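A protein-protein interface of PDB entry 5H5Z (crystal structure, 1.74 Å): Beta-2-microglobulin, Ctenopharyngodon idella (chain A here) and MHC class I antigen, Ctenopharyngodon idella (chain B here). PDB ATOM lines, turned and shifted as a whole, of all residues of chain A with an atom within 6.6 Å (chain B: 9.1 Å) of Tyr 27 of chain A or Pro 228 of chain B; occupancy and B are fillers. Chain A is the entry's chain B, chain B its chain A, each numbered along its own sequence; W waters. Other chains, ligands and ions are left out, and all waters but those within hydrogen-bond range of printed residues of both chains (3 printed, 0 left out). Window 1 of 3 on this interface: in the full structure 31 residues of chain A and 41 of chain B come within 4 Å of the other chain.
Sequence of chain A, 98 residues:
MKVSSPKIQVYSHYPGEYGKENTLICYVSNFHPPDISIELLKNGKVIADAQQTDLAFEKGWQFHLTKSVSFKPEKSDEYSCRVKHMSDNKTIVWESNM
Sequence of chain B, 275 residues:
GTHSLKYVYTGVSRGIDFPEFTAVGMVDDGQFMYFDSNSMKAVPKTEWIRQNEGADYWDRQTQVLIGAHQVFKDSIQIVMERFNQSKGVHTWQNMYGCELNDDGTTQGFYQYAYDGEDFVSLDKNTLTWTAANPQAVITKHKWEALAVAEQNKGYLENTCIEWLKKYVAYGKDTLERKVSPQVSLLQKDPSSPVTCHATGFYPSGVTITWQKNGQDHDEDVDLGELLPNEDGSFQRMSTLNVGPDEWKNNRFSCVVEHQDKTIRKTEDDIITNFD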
ATOM      1  N   LYS A   7       8.147   0.358  15.937  1.00  0.00           N
ATOM      2  CA  LYS A   7       7.673  -0.985  15.626  1.00  0.00           C
ATOM      3  C   LYS A   7       8.726  -1.926  16.198  1.00  0.00           C
ATOM      4  O   LYS A   7       9.929  -1.684  16.046  1.00  0.00           O
ATOM      5  CB  LYS A   7       7.527  -1.192  14.118  1.00  0.00           C
ATOM      6  CG  LYS A   7       6.848  -2.504  13.736  1.00  0.00           C
ATOM      7  CD  LYS A   7       7.071  -2.869  12.277  1.00  0.00           C
ATOM      8  CE  LYS A   7       6.112  -2.155  11.339  1.00  0.00           C
ATOM      9  NZ  LYS A   7       6.597  -2.253   9.931  1.00  0.00           N
ATOM     10  N   ILE A   8       8.271  -2.972  16.880  1.00  0.00           N
ATOM     11  CA  ILE A   8       9.160  -3.905  17.571  1.00  0.00           C
ATOM     12  C   ILE A   8       8.842  -5.324  17.140  1.00  0.00           C
ATOM     13  O   ILE A   8       7.727  -5.815  17.351  1.00  0.00           O
ATOM     14  CB  ILE A   8       9.011  -3.812  19.107  1.00  0.00           C
ATOM     15  CG1 ILE A   8       9.175  -2.363  19.579  1.00  0.00           C
ATOM     16  CG2 ILE A   8      10.014  -4.734  19.795  1.00  0.00           C
ATOM     17  CD1 ILE A   8       8.698  -2.113  20.993  1.00  0.00           C
ATOM     18  N   GLN A   9       9.824  -5.980  16.537  1.00  0.00           N
ATOM     19  CA  GLN A   9       9.640  -7.327  16.023  1.00  0.00           C
ATOM     20  C   GLN A   9      10.734  -8.230  16.560  1.00  0.00           C
ATOM     21  O   GLN A   9      11.930  -7.933  16.421  1.00  0.00           O
ATOM     22  CB  GLN A   9       9.606  -7.329  14.493  1.00  0.00           C
ATOM     23  CG  GLN A   9       8.409  -6.581  13.921  1.00  0.00           C
ATOM     24  CD  GLN A   9       8.448  -6.458  12.413  1.00  0.00           C
ATOM     25  OE1 GLN A   9       7.754  -7.185  11.699  1.00  0.00           O
ATOM     26  NE2 GLN A   9       9.256  -5.538  11.919  1.00  0.00           N
ATOM     27  N   VAL A  10      10.303  -9.328  17.177  1.00  0.00           N
ATOM     28  CA  VAL A  10      11.196 -10.258  17.865  1.00  0.00           C
ATOM     29  C   VAL A  10      11.079 -11.625  17.205  1.00  0.00           C
ATOM     30  O   VAL A  10       9.979 -12.175  17.083  1.00  0.00           O
ATOM     31  CB  VAL A  10      10.865 -10.356  19.376  1.00  0.00           C
ATOM     32  CG1 VAL A  10      11.951 -11.124  20.123  1.00  0.00           C
ATOM     33  CG2 VAL A  10      10.703  -8.971  19.973  1.00  0.00           C
ATOM     34  N   TYR A  11      12.217 -12.152  16.763  1.00  0.00           N
ATOM     35  CA  TYR A  11      12.261 -13.389  15.991  1.00  0.00           C
ATOM     36  C   TYR A  11      13.638 -14.028  16.098  1.00  0.00           C
ATOM     37  O   TYR A  11      14.575 -13.432  16.631  1.00  0.00           O
ATOM     38  CB  TYR A  11      11.899 -13.124  14.518  1.00  0.00           C
ATOM     39  CG  TYR A  11      12.673 -11.992  13.866  1.00  0.00           C
ATOM     40  CD1 TYR A  11      12.299 -10.662  14.058  1.00  0.00           C
ATOM     41  CD2 TYR A  11      13.771 -12.256  13.041  1.00  0.00           C
ATOM     42  CE1 TYR A  11      13.004  -9.625  13.464  1.00  0.00           C
ATOM     43  CE2 TYR A  11      14.481 -11.226  12.432  1.00  0.00           C
ATOM     44  CZ  TYR A  11      14.093  -9.911  12.650  1.00  0.00           C
ATOM     45  OH  TYR A  11      14.776  -8.873  12.064  1.00  0.00           O
ATOM     46  N   ILE A  25      16.752 -12.136  17.652  1.00  0.00           N
ATOM     47  CA  ILE A  25      16.818 -10.842  16.985  1.00  0.00           C
ATOM     48  C   ILE A  25      15.635  -9.965  17.367  1.00  0.00           C
ATOM     49  O   ILE A  25      14.474 -10.410  17.348  1.00  0.00           O
ATOM     50  CB  ILE A  25      16.860 -11.006  15.444  1.00  0.00           C
ATOM     51  CG1 ILE A  25      18.057 -11.876  15.026  1.00  0.00           C
ATOM     52  CG2 ILE A  25      16.875  -9.644  14.758  1.00  0.00           C
ATOM     53  CD1 ILE A  25      17.990 -12.399  13.605  1.00  0.00           C
ATOM     54  N   CYS A  26      15.932  -8.716  17.721  1.00  0.00           N
ATOM     55  CA  CYS A  26      14.896  -7.725  17.943  1.00  0.00           C
ATOM     56  C   CYS A  26      15.119  -6.555  16.989  1.00  0.00           C
ATOM     57  O   CYS A  26      16.095  -5.820  17.119  1.00  0.00           O
ATOM     58  CB  CYS A  26      14.890  -7.278  19.405  1.00  0.00           C
ATOM     59  SG  CYS A  26      13.616  -6.078  19.836  1.00  0.00           S
ATOM     60  N   TYR A  27      14.218  -6.420  16.018  1.00  0.00           N
ATOM     61  CA  TYR A  27      14.267  -5.349  15.029  1.00  0.00           C
ATOM     62  C   TYR A  27      13.338  -4.224  15.450  1.00  0.00           C
ATOM     63  O   TYR A  27      12.117  -4.409  15.548  1.00  0.00           O
ATOM     64  CB  TYR A  27      13.866  -5.876  13.652  1.00  0.00           C
ATOM     65  CG  TYR A  27      13.958  -4.865  12.525  1.00  0.00           C
ATOM     66  CD1 TYR A  27      15.121  -4.112  12.317  1.00  0.00           C
ATOM     67  CD2 TYR A  27      12.900  -4.694  11.637  1.00  0.00           C
ATOM     68  CE1 TYR A  27      15.201  -3.199  11.276  1.00  0.00           C
ATOM     69  CE2 TYR A  27      12.973  -3.792  10.591  1.00  0.00           C
ATOM     70  CZ  TYR A  27      14.122  -3.046  10.416  1.00  0.00           C
ATOM     71  OH  TYR A  27      14.186  -2.150   9.376  1.00  0.00           O
ATOM     72  N   VAL A  28      13.932  -3.064  15.708  1.00  0.00           N
ATOM     73  CA  VAL A  28      13.201  -1.904  16.213  1.00  0.00           C
ATOM     74  C   VAL A  28      13.259  -0.817  15.143  1.00  0.00           C
ATOM     75  O   VAL A  28      14.339  -0.332  14.806  1.00  0.00           O
ATOM     76  CB  VAL A  28      13.796  -1.425  17.555  1.00  0.00           C
ATOM     77  CG1 VAL A  28      13.027  -0.227  18.100  1.00  0.00           C
ATOM     78  CG2 VAL A  28      13.796  -2.562  18.573  1.00  0.00           C
ATOM     79  N   SER A  29      12.105  -0.452  14.590  1.00  0.00           N
ATOM     80  CA  SER A  29      12.081   0.395  13.399  1.00  0.00           C
ATOM     81  C   SER A  29      11.016   1.478  13.469  1.00  0.00           C
ATOM     82  O   SER A  29      10.211   1.501  14.397  1.00  0.00           O
ATOM     83  CB  SER A  29      11.857  -0.466  12.156  1.00  0.00           C
ATOM     84  OG  SER A  29      10.585  -1.103  12.216  1.00  0.00           O
ATOM     85  N   ASN A  30      11.027   2.374  12.483  1.00  0.00           N
ATOM     86  CA  ASN A  30       9.988   3.395  12.328  1.00  0.00           C
ATOM     87  C   ASN A  30       9.877   4.361  13.513  1.00  0.00           C
ATOM     88  O   ASN A  30       8.780   4.818  13.841  1.00  0.00           O
ATOM     89  CB  ASN A  30       8.619   2.740  12.053  1.00  0.00           C
ATOM     90  CG  ASN A  30       8.577   1.979  10.737  1.00  0.00           C
ATOM     91  OD1 ASN A  30       9.431   2.158   9.864  1.00  0.00           O
ATOM     92  ND2 ASN A  30       7.569   1.126  10.586  1.00  0.00           N
ATOM     93  N   ILE A  38      17.265  -0.585  24.069  1.00  0.00           N
ATOM     94  CA  ILE A  38      16.829  -1.921  23.659  1.00  0.00           C
ATOM     95  C   ILE A  38      17.622  -2.965  24.441  1.00  0.00           C
ATOM     96  O   ILE A  38      18.853  -2.904  24.493  1.00  0.00           O
ATOM     97  CB  ILE A  38      17.013  -2.165  22.139  1.00  0.00           C
ATOM     98  CG1 ILE A  38      16.347  -1.060  21.309  1.00  0.00           C
ATOM     99  CG2 ILE A  38      16.467  -3.538  21.751  1.00  0.00           C
ATOM    100  CD1 ILE A  38      16.837  -0.983  19.876  1.00  0.00           C
ATOM    101  N   GLU A  58      15.965   5.215   7.352  1.00  0.00           N
ATOM    102  CA  GLU A  58      15.538   4.938   5.989  1.00  0.00           C
ATOM    103  C   GLU A  58      14.997   6.202   5.341  1.00  0.00           C
ATOM    104  O   GLU A  58      14.945   7.260   5.976  1.00  0.00           O
ATOM    105  CB  GLU A  58      14.458   3.851   5.998  1.00  0.00           C
ATOM    106  CG  GLU A  58      14.970   2.474   6.394  1.00  0.00           C
ATOM    107  CD  GLU A  58      13.858   1.458   6.554  1.00  0.00           C
ATOM    108  OE1 GLU A  58      12.958   1.672   7.394  1.00  0.00           O
ATOM    109  OE2 GLU A  58      13.891   0.433   5.842  1.00  0.00           O
ATOM    110  N   HIS A  64      16.049   2.966  12.576  1.00  0.00           N
ATOM    111  CA  HIS A  64      15.922   1.536  12.832  1.00  0.00           C
ATOM    112  C   HIS A  64      17.192   1.005  13.484  1.00  0.00           C
ATOM    113  O   HIS A  64      18.299   1.487  13.206  1.00  0.00           O
ATOM    114  CB  HIS A  64      15.568   0.755  11.558  1.00  0.00           C
ATOM    115  CG  HIS A  64      16.626   0.808  10.495  1.00  0.00           C
ATOM    116  ND1 HIS A  64      17.499  -0.232  10.261  1.00  0.00           N
ATOM    117  CD2 HIS A  64      16.943   1.774   9.601  1.00  0.00           C
ATOM    118  CE1 HIS A  64      18.310   0.092   9.269  1.00  0.00           C
ATOM    119  NE2 HIS A  64      17.994   1.305   8.852  1.00  0.00           N
ATOM    120  N   LEU A  65      17.015   0.043  14.383  1.00  0.00           N
ATOM    121  CA  LEU A  65      18.125  -0.633  15.039  1.00  0.00           C
ATOM    122  C   LEU A  65      17.832  -2.114  15.153  1.00  0.00           C
ATOM    123  O   LEU A  65      16.676  -2.524  15.251  1.00  0.00           O
ATOM    124  CB  LEU A  65      18.355  -0.074  16.445  1.00  0.00           C
ATOM    125  CG  LEU A  65      18.869   1.356  16.596  1.00  0.00           C
ATOM    126  CD1 LEU A  65      18.662   1.824  18.024  1.00  0.00           C
ATOM    127  CD2 LEU A  65      20.342   1.472  16.201  1.00  0.00           C
ATOM    128  N   THR A  66      18.888  -2.914  15.143  1.00  0.00           N
ATOM    129  CA  THR A  66      18.764  -4.344  15.372  1.00  0.00           C
ATOM    130  C   THR A  66      19.617  -4.740  16.573  1.00  0.00           C
ATOM    131  O   THR A  66      20.809  -4.441  16.623  1.00  0.00           O
ATOM    132  CB  THR A  66      19.170  -5.155  14.125  1.00  0.00           C
ATOM    133  OG1 THR A  66      18.384  -4.733  13.004  1.00  0.00           O
ATOM    134  CG2 THR A  66      18.951  -6.647  14.350  1.00  0.00           C
ATOM    135  N   LYS A  67      18.990  -5.383  17.554  1.00  0.00           N
ATOM    136  CA  LYS A  67      19.726  -6.004  18.645  1.00  0.00           C
ATOM    137  C   LYS A  67      19.630  -7.510  18.497  1.00  0.00           C
ATOM    138  O   LYS A  67      18.564  -8.035  18.186  1.00  0.00           O
ATOM    139  CB  LYS A  67      19.191  -5.568  20.002  1.00  0.00           C
ATOM    140  CG  LYS A  67      20.145  -5.884  21.138  1.00  0.00           C
ATOM    141  CD  LYS A  67      20.194  -4.719  22.101  1.00  0.00           C
ATOM    142  CE  LYS A  67      21.455  -4.722  22.935  1.00  0.00           C
ATOM    143  NZ  LYS A  67      21.453  -3.556  23.860  1.00  0.00           N
ATOM    144  N   CYS A  81      12.124  -8.884  24.252  1.00  0.00           N
ATOM    145  CA  CYS A  81      12.857  -7.673  23.933  1.00  0.00           C
ATOM    146  C   CYS A  81      12.137  -6.513  24.603  1.00  0.00           C
ATOM    147  O   CYS A  81      10.934  -6.315  24.388  1.00  0.00           O
ATOM    148  CB  CYS A  81      12.929  -7.478  22.415  1.00  0.00           C
ATOM    149  SG  CYS A  81      13.751  -5.966  21.864  1.00  0.00           S
ATOM    150  N   ASP B  29      23.041  -0.760   0.848  1.00  0.00           N
ATOM    151  CA  ASP B  29      22.355  -0.690   2.144  1.00  0.00           C
ATOM    152  C   ASP B  29      23.000  -1.525   3.248  1.00  0.00           C
ATOM    153  O   ASP B  29      22.393  -1.764   4.296  1.00  0.00           O
ATOM    154  CB  ASP B  29      20.861  -0.998   1.974  1.00  0.00           C
ATOM    155  CG  ASP B  29      20.199  -0.077   0.966  1.00  0.00           C
ATOM    156  OD1 ASP B  29      20.223   1.152   1.182  1.00  0.00           O
ATOM    157  OD2 ASP B  29      19.666  -0.573  -0.046  1.00  0.00           O
ATOM    158  N   ALA B 198      11.392 -18.707   5.533  1.00  0.00           N
ATOM    159  CA  ALA B 198      12.574 -18.652   4.666  1.00  0.00           C
ATOM    160  C   ALA B 198      13.605 -17.735   5.295  1.00  0.00           C
ATOM    161  O   ALA B 198      13.284 -16.598   5.650  1.00  0.00           O
ATOM    162  CB  ALA B 198      12.192 -18.143   3.285  1.00  0.00           C
ATOM    163  N   THR B 199      14.842 -18.215   5.428  1.00  0.00           N
ATOM    164  CA  THR B 199      15.890 -17.428   6.085  1.00  0.00           C
ATOM    165  C   THR B 199      17.269 -17.597   5.444  1.00  0.00           C
ATOM    166  O   THR B 199      17.543 -18.608   4.790  1.00  0.00           O
ATOM    167  CB  THR B 199      15.986 -17.737   7.599  1.00  0.00           C
ATOM    168  OG1 THR B 199      16.741 -16.707   8.254  1.00  0.00           O
ATOM    169  CG2 THR B 199      16.644 -19.100   7.864  1.00  0.00           C
ATOM    170  N   GLY B 200      18.128 -16.602   5.646  1.00  0.00           N
ATOM    171  CA  GLY B 200      19.533 -16.702   5.271  1.00  0.00           C
ATOM    172  C   GLY B 200      19.829 -16.357   3.829  1.00  0.00           C
ATOM    173  O   GLY B 200      20.906 -16.660   3.325  1.00  0.00           O
ATOM    174  N   PHE B 201      18.878 -15.714   3.165  1.00  0.00           N
ATOM    175  CA  PHE B 201      19.013 -15.437   1.744  1.00  0.00           C
ATOM    176  C   PHE B 201      19.515 -14.020   1.445  1.00  0.00           C
ATOM    177  O   PHE B 201      19.330 -13.087   2.234  1.00  0.00           O
ATOM    178  CB  PHE B 201      17.705 -15.744   0.993  1.00  0.00           C
ATOM    179  CG  PHE B 201      16.505 -15.007   1.521  1.00  0.00           C
ATOM    180  CD1 PHE B 201      16.199 -13.729   1.065  1.00  0.00           C
ATOM    181  CD2 PHE B 201      15.669 -15.598   2.474  1.00  0.00           C
ATOM    182  CE1 PHE B 201      15.086 -13.053   1.548  1.00  0.00           C
ATOM    183  CE2 PHE B 201      14.561 -14.922   2.963  1.00  0.00           C
ATOM    184  CZ  PHE B 201      14.270 -13.646   2.502  1.00  0.00           C
ATOM    185  N   SER B 204      17.652  -9.519  -1.116  1.00  0.00           N
ATOM    186  CA  SER B 204      16.487  -9.554  -0.224  1.00  0.00           C
ATOM    187  C   SER B 204      15.154  -9.962  -0.858  1.00  0.00           C
ATOM    188  O   SER B 204      14.241 -10.384  -0.145  1.00  0.00           O
ATOM    189  CB  SER B 204      16.337  -8.217   0.506  1.00  0.00           C
ATOM    190  OG  SER B 204      15.859  -7.225  -0.378  1.00  0.00           O
ATOM    191  N   GLU B 225       6.445  -9.526   6.773  1.00  0.00           N
ATOM    192  CA  GLU B 225       7.348  -8.527   6.208  1.00  0.00           C
ATOM    193  C   GLU B 225       8.736  -9.115   5.998  1.00  0.00           C
ATOM    194  O   GLU B 225       9.118 -10.078   6.668  1.00  0.00           O
ATOM    195  CB  GLU B 225       7.432  -7.302   7.122  1.00  0.00           C
ATOM    196  CG  GLU B 225       6.086  -6.631   7.379  1.00  0.00           C
ATOM    197  CD  GLU B 225       6.141  -5.560   8.453  1.00  0.00           C
ATOM    198  OE1 GLU B 225       5.184  -4.762   8.535  1.00  0.00           O
ATOM    199  OE2 GLU B 225       7.131  -5.509   9.215  1.00  0.00           O
ATOM    200  N   LEU B 226       9.478  -8.533   5.059  1.00  0.00           N
ATOM    201  CA  LEU B 226      10.905  -8.802   4.915  1.00  0.00           C
ATOM    202  C   LEU B 226      11.614  -8.325   6.177  1.00  0.00           C
ATOM    203  O   LEU B 226      11.410  -7.186   6.616  1.00  0.00           O
ATOM    204  CB  LEU B 226      11.468  -8.081   3.680  1.00  0.00           C
ATOM    205  CG  LEU B 226      12.967  -8.186   3.378  1.00  0.00           C
ATOM    206  CD1 LEU B 226      13.379  -9.607   3.007  1.00  0.00           C
ATOM    207  CD2 LEU B 226      13.353  -7.226   2.263  1.00  0.00           C
ATOM    208  N   LEU B 227      12.435  -9.192   6.763  1.00  0.00           N
ATOM    209  CA  LEU B 227      13.126  -8.861   8.007  1.00  0.00           C
ATOM    210  C   LEU B 227      14.618  -9.115   7.901  1.00  0.00           C
ATOM    211  O   LEU B 227      15.033 -10.086   7.267  1.00  0.00           O
ATOM    212  CB  LEU B 227      12.572  -9.678   9.171  1.00  0.00           C
ATOM    213  CG  LEU B 227      11.119  -9.486   9.601  1.00  0.00           C
ATOM    214  CD1 LEU B 227      10.734 -10.572  10.592  1.00  0.00           C
ATOM    215  CD2 LEU B 227      10.889  -8.103  10.200  1.00  0.00           C
ATOM    216  N   PRO B 228      15.431  -8.253   8.539  1.00  0.00           N
ATOM    217  CA  PRO B 228      16.872  -8.459   8.504  1.00  0.00           C
ATOM    218  C   PRO B 228      17.343  -9.492   9.520  1.00  0.00           C
ATOM    219  O   PRO B 228      16.852  -9.536  10.655  1.00  0.00           O
ATOM    220  CB  PRO B 228      17.425  -7.083   8.876  1.00  0.00           C
ATOM    221  CG  PRO B 228      16.385  -6.507   9.778  1.00  0.00           C
ATOM    222  CD  PRO B 228      15.068  -7.005   9.245  1.00  0.00           C
ATOM    223  N   ASN B 229      18.292 -10.324   9.109  1.00  0.00           N
ATOM    224  CA  ASN B 229      19.040 -11.121  10.067  1.00  0.00           C
ATOM    225  C   ASN B 229      20.208 -10.297  10.619  1.00  0.00           C
ATOM    226  O   ASN B 229      20.406  -9.147  10.219  1.00  0.00           O
ATOM    227  CB  ASN B 229      19.508 -12.433   9.436  1.00  0.00           C
ATOM    228  CG  ASN B 229      18.392 -13.458   9.333  1.00  0.00           C
ATOM    229  OD1 ASN B 229      17.495 -13.504  10.185  1.00  0.00           O
ATOM    230  ND2 ASN B 229      18.436 -14.286   8.293  1.00  0.00           N
ATOM    231  N   GLU B 230      20.972 -10.889  11.533  1.00  0.00           N
ATOM    232  CA  GLU B 230      22.080 -10.210  12.203  1.00  0.00           C
ATOM    233  C   GLU B 230      23.345 -10.122  11.345  1.00  0.00           C
ATOM    234  O   GLU B 230      24.250  -9.346  11.655  1.00  0.00           O
ATOM    235  CB  GLU B 230      22.394 -10.904  13.537  1.00  0.00           C
ATOM    236  CG  GLU B 230      23.325 -12.117  13.465  1.00  0.00           C
ATOM    237  CD  GLU B 230      22.698 -13.367  12.851  1.00  0.00           C
ATOM    238  OE1 GLU B 230      23.441 -14.348  12.636  1.00  0.00           O
ATOM    239  OE2 GLU B 230      21.479 -13.388  12.580  1.00  0.00           O
ATOM    240  N   ASP B 231      23.389 -10.908  10.270  1.00  0.00           N
ATOM    241  CA  ASP B 231      24.615 -11.134   9.503  1.00  0.00           C
ATOM    242  C   ASP B 231      24.574 -10.573   8.081  1.00  0.00           C
ATOM    243  O   ASP B 231      25.436 -10.897   7.260  1.00  0.00           O
ATOM    244  CB  ASP B 231      24.933 -12.640   9.466  1.00  0.00           C
ATOM    245  CG  ASP B 231      23.856 -13.459   8.749  1.00  0.00           C
ATOM    246  OD1 ASP B 231      22.807 -12.897   8.370  1.00  0.00           O
ATOM    247  OD2 ASP B 231      24.064 -14.674   8.558  1.00  0.00           O
ATOM    248  N   GLY B 232      23.573  -9.744   7.786  1.00  0.00           N
ATOM    249  CA  GLY B 232      23.430  -9.161   6.450  1.00  0.00           C
ATOM    250  C   GLY B 232      22.517  -9.939   5.517  1.00  0.00           C
ATOM    251  O   GLY B 232      22.163  -9.450   4.440  1.00  0.00           O
ATOM    252  N   SER B 233      22.139 -11.151   5.921  1.00  0.00           N
ATOM    253  CA  SER B 233      21.133 -11.912   5.187  1.00  0.00           C
ATOM    254  C   SER B 233      19.737 -11.491   5.630  1.00  0.00           C
ATOM    255  O   SER B 233      19.583 -10.653   6.523  1.00  0.00           O
ATOM    256  CB  SER B 233      21.326 -13.426   5.362  1.00  0.00           C
ATOM    257  OG  SER B 233      20.967 -13.855   6.668  1.00  0.00           O
ATOM    258  N   PHE B 234      18.726 -12.076   5.000  1.00  0.00           N
ATOM    259  CA  PHE B 234      17.340 -11.703   5.248  1.00  0.00           C
ATOM    260  C   PHE B 234      16.470 -12.907   5.522  1.00  0.00           C
ATOM    261  O   PHE B 234      16.867 -14.044   5.244  1.00  0.00           O
ATOM    262  CB  PHE B 234      16.794 -10.942   4.047  1.00  0.00           C
ATOM    263  CG  PHE B 234      17.418  -9.599   3.874  1.00  0.00           C
ATOM    264  CD1 PHE B 234      18.570  -9.440   3.103  1.00  0.00           C
ATOM    265  CD2 PHE B 234      16.879  -8.494   4.518  1.00  0.00           C
ATOM    266  CE1 PHE B 234      19.160  -8.192   2.956  1.00  0.00           C
ATOM    267  CE2 PHE B 234      17.465  -7.240   4.380  1.00  0.00           C
ATOM    268  CZ  PHE B 234      18.605  -7.090   3.599  1.00  0.00           C
ATOM    269  N   GLN B 235      15.285 -12.650   6.072  1.00  0.00           N
ATOM    270  CA  GLN B 235      14.287 -13.701   6.248  1.00  0.00           C
ATOM    271  C   GLN B 235      12.892 -13.158   5.975  1.00  0.00           C
ATOM    272  O   GLN B 235      12.677 -11.943   5.981  1.00  0.00           O
ATOM    273  CB  GLN B 235      14.383 -14.325   7.646  1.00  0.00           C
ATOM    274  CG  GLN B 235      14.017 -13.410   8.804  1.00  0.00           C
ATOM    275  CD  GLN B 235      13.790 -14.191  10.080  1.00  0.00           C
ATOM    276  OE1 GLN B 235      12.655 -14.513  10.424  1.00  0.00           O
ATOM    277  NE2 GLN B 235      14.872 -14.534  10.771  1.00  0.00           N
ATOM    278  N   ARG B 236      11.958 -14.068   5.716  1.00  0.00           N
ATOM    279  CA  ARG B 236      10.552 -13.734   5.500  1.00  0.00           C
ATOM    280  C   ARG B 236       9.725 -14.992   5.715  1.00  0.00           C
ATOM    281  O   ARG B 236      10.204 -16.109   5.491  1.00  0.00           O
ATOM    282  CB  ARG B 236      10.325 -13.192   4.084  1.00  0.00           C
ATOM    283  CG  ARG B 236       9.041 -12.400   3.924  1.00  0.00           C
ATOM    284  CD  ARG B 236       8.986 -11.645   2.606  1.00  0.00           C
ATOM    285  NE  ARG B 236       7.808 -10.780   2.559  1.00  0.00           N
ATOM    286  CZ  ARG B 236       7.591  -9.838   1.647  1.00  0.00           C
ATOM    287  NH1 ARG B 236       8.476  -9.618   0.682  1.00  0.00           N
ATOM    288  NH2 ARG B 236       6.484  -9.108   1.704  1.00  0.00           N
HETATM  289  O   HOH W   1       9.547  -4.406   9.498  1.00  0.00           O
HETATM  290  O   HOH W   2      20.566  -6.137  10.906  1.00  0.00           O
HETATM  291  O   HOH W   3       6.146  -9.200   9.587  1.00  0.00           O
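NZ of Lys 7 of chain A lies within salt-bridge range of OE1 of Glu 225 of chain B (3.2 Å). The side-chain carboxylate (OE2) of Glu 225 of chain B sits close to the side-chain amide oxygen (OE1) of Gln 9 of chain A. The backbone carbonyl oxygen (O) of Pro 228 of chain B lies within hydrogen-bond range of the side-chain hydroxyl (OH) of Tyr 11 of chain A, at 2.6 Å.
ND2 of Asn 229 of chain B is in hydrogen-bond range of OG1 of Thr 199 of chain B. The side-chain amide nitrogen (ND2) of Asn 229 of chain B is in hydrogen-bond range of the backbone carbonyl oxygen (O) of Phe 234 of chain B (3.4 Å). The side-chain amide nitrogen (NE2) of Gln 235 of chain B sits at hydrogen-bond distance from the side-chain amide oxygen (OD1) of Asn 229 of chain B, at 2.9 Å. The backbone carbonyl oxygen (O) of Ser 29 of chain A lies within hydrogen-bond range of the backbone NH (N) of Lys 7 of chain A (2.8 Å). O of Gln 9 of chain A sits at hydrogen-bond distance from N of Tyr 27 of chain A, at 2.8 Å. The backbone carbonyl oxygen (O) of Tyr 11 of chain A sits at hydrogen-bond distance from the backbone NH (N) of Ile 25 of chain A (2.7 Å).
Gln 9 of chain A touches Leu 227 of chain B (NE2 to CD2, 3.5 Å). Leu 227 of chain B touches Tyr 11 of chain A. Tyr 11 of chain A touches Gln 235 of chain B (CD2 to NE2, 3.4 Å). Asn 229 of chain B touches Ile 25 of chain A (OD1 to CD1, 3.6 Å). OE2 of Glu 230 of chain B touches CD1 of Ile 25 of chain A, 3.8 Å away. CD1 of Tyr 27 of chain A touches CG of Pro 228 of chain B, 3.7 Å away.
Of chain B, only Pro 228 (3.7 Å) comes within 4 Å of Tyr 27 of chain A. Pro 228 of chain B touches two residues of chain A. No residue of chain B comes within 4 Å of Cys 26 of chain A. Val 28 of chain A touches none of the printed residues of chain B. Printed residues of chain A within 4 Å of Gln 235 of chain B: Tyr 11. Of the printed residues of chain B, Tyr 11 of chain A touches Leu 227, Pro 228 and Gln 235. Printed residues of chain A within 4 Å of Glu 230 of chain B: Ile 25. Of the printed residues of chain A, Asn 229 of chain B touches Ile 25 (3.6 Å). Printed residues of chain B within 4 Å of Ile 25 of chain A: Asn 229 (3.6 Å) and Glu 230 (3.8 Å). Gly 232 of chain B touches none of the printed residues of chain A. The nearest residue of chain B that does not touch Tyr 27 of chain A is Leu 227 of chain B (4.2 Å). The nearest residue of chain A that does not touch Pro 228 of chain B is Ile 25 of chain A (4.1 Å).
Of the 18 printed residues of chain B, 6 touch a printed residue of chain A. Printed residues of chain B that touch a printed residue of chain A: Glu 225, Leu 227, Pro 228, Asn 229, Glu 230 and Gln 235. Along chain B the printed residues that touch a printed residue of chain A span positions 225 to 235. Among the printed residues, 9 pairs touch across the chains. Among the printed residues, Asp or Glu carboxylates within 4 Å of a Lys or Arg side-chain nitrogen of the other chain: Lys 7 of chain A with Glu 225 of chain B (3.2 Å).
Water W1 bridges the side-chain carboxylate (OE2) of Glu 225 of chain B (2.7 Å) and the side-chain amide nitrogen (NE2) of Gln 9 of chain A (2.7 Å). Water W3 lies within hydrogen-bond range of N of Glu 225 of chain B (2.8 Å) and OE1 of Gln 9 of chain A (3.3 Å). Water W2 bridges O of Asn 229 of chain B (3.1 Å) and OG1 of Thr 66 of chain A (3.3 Å).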
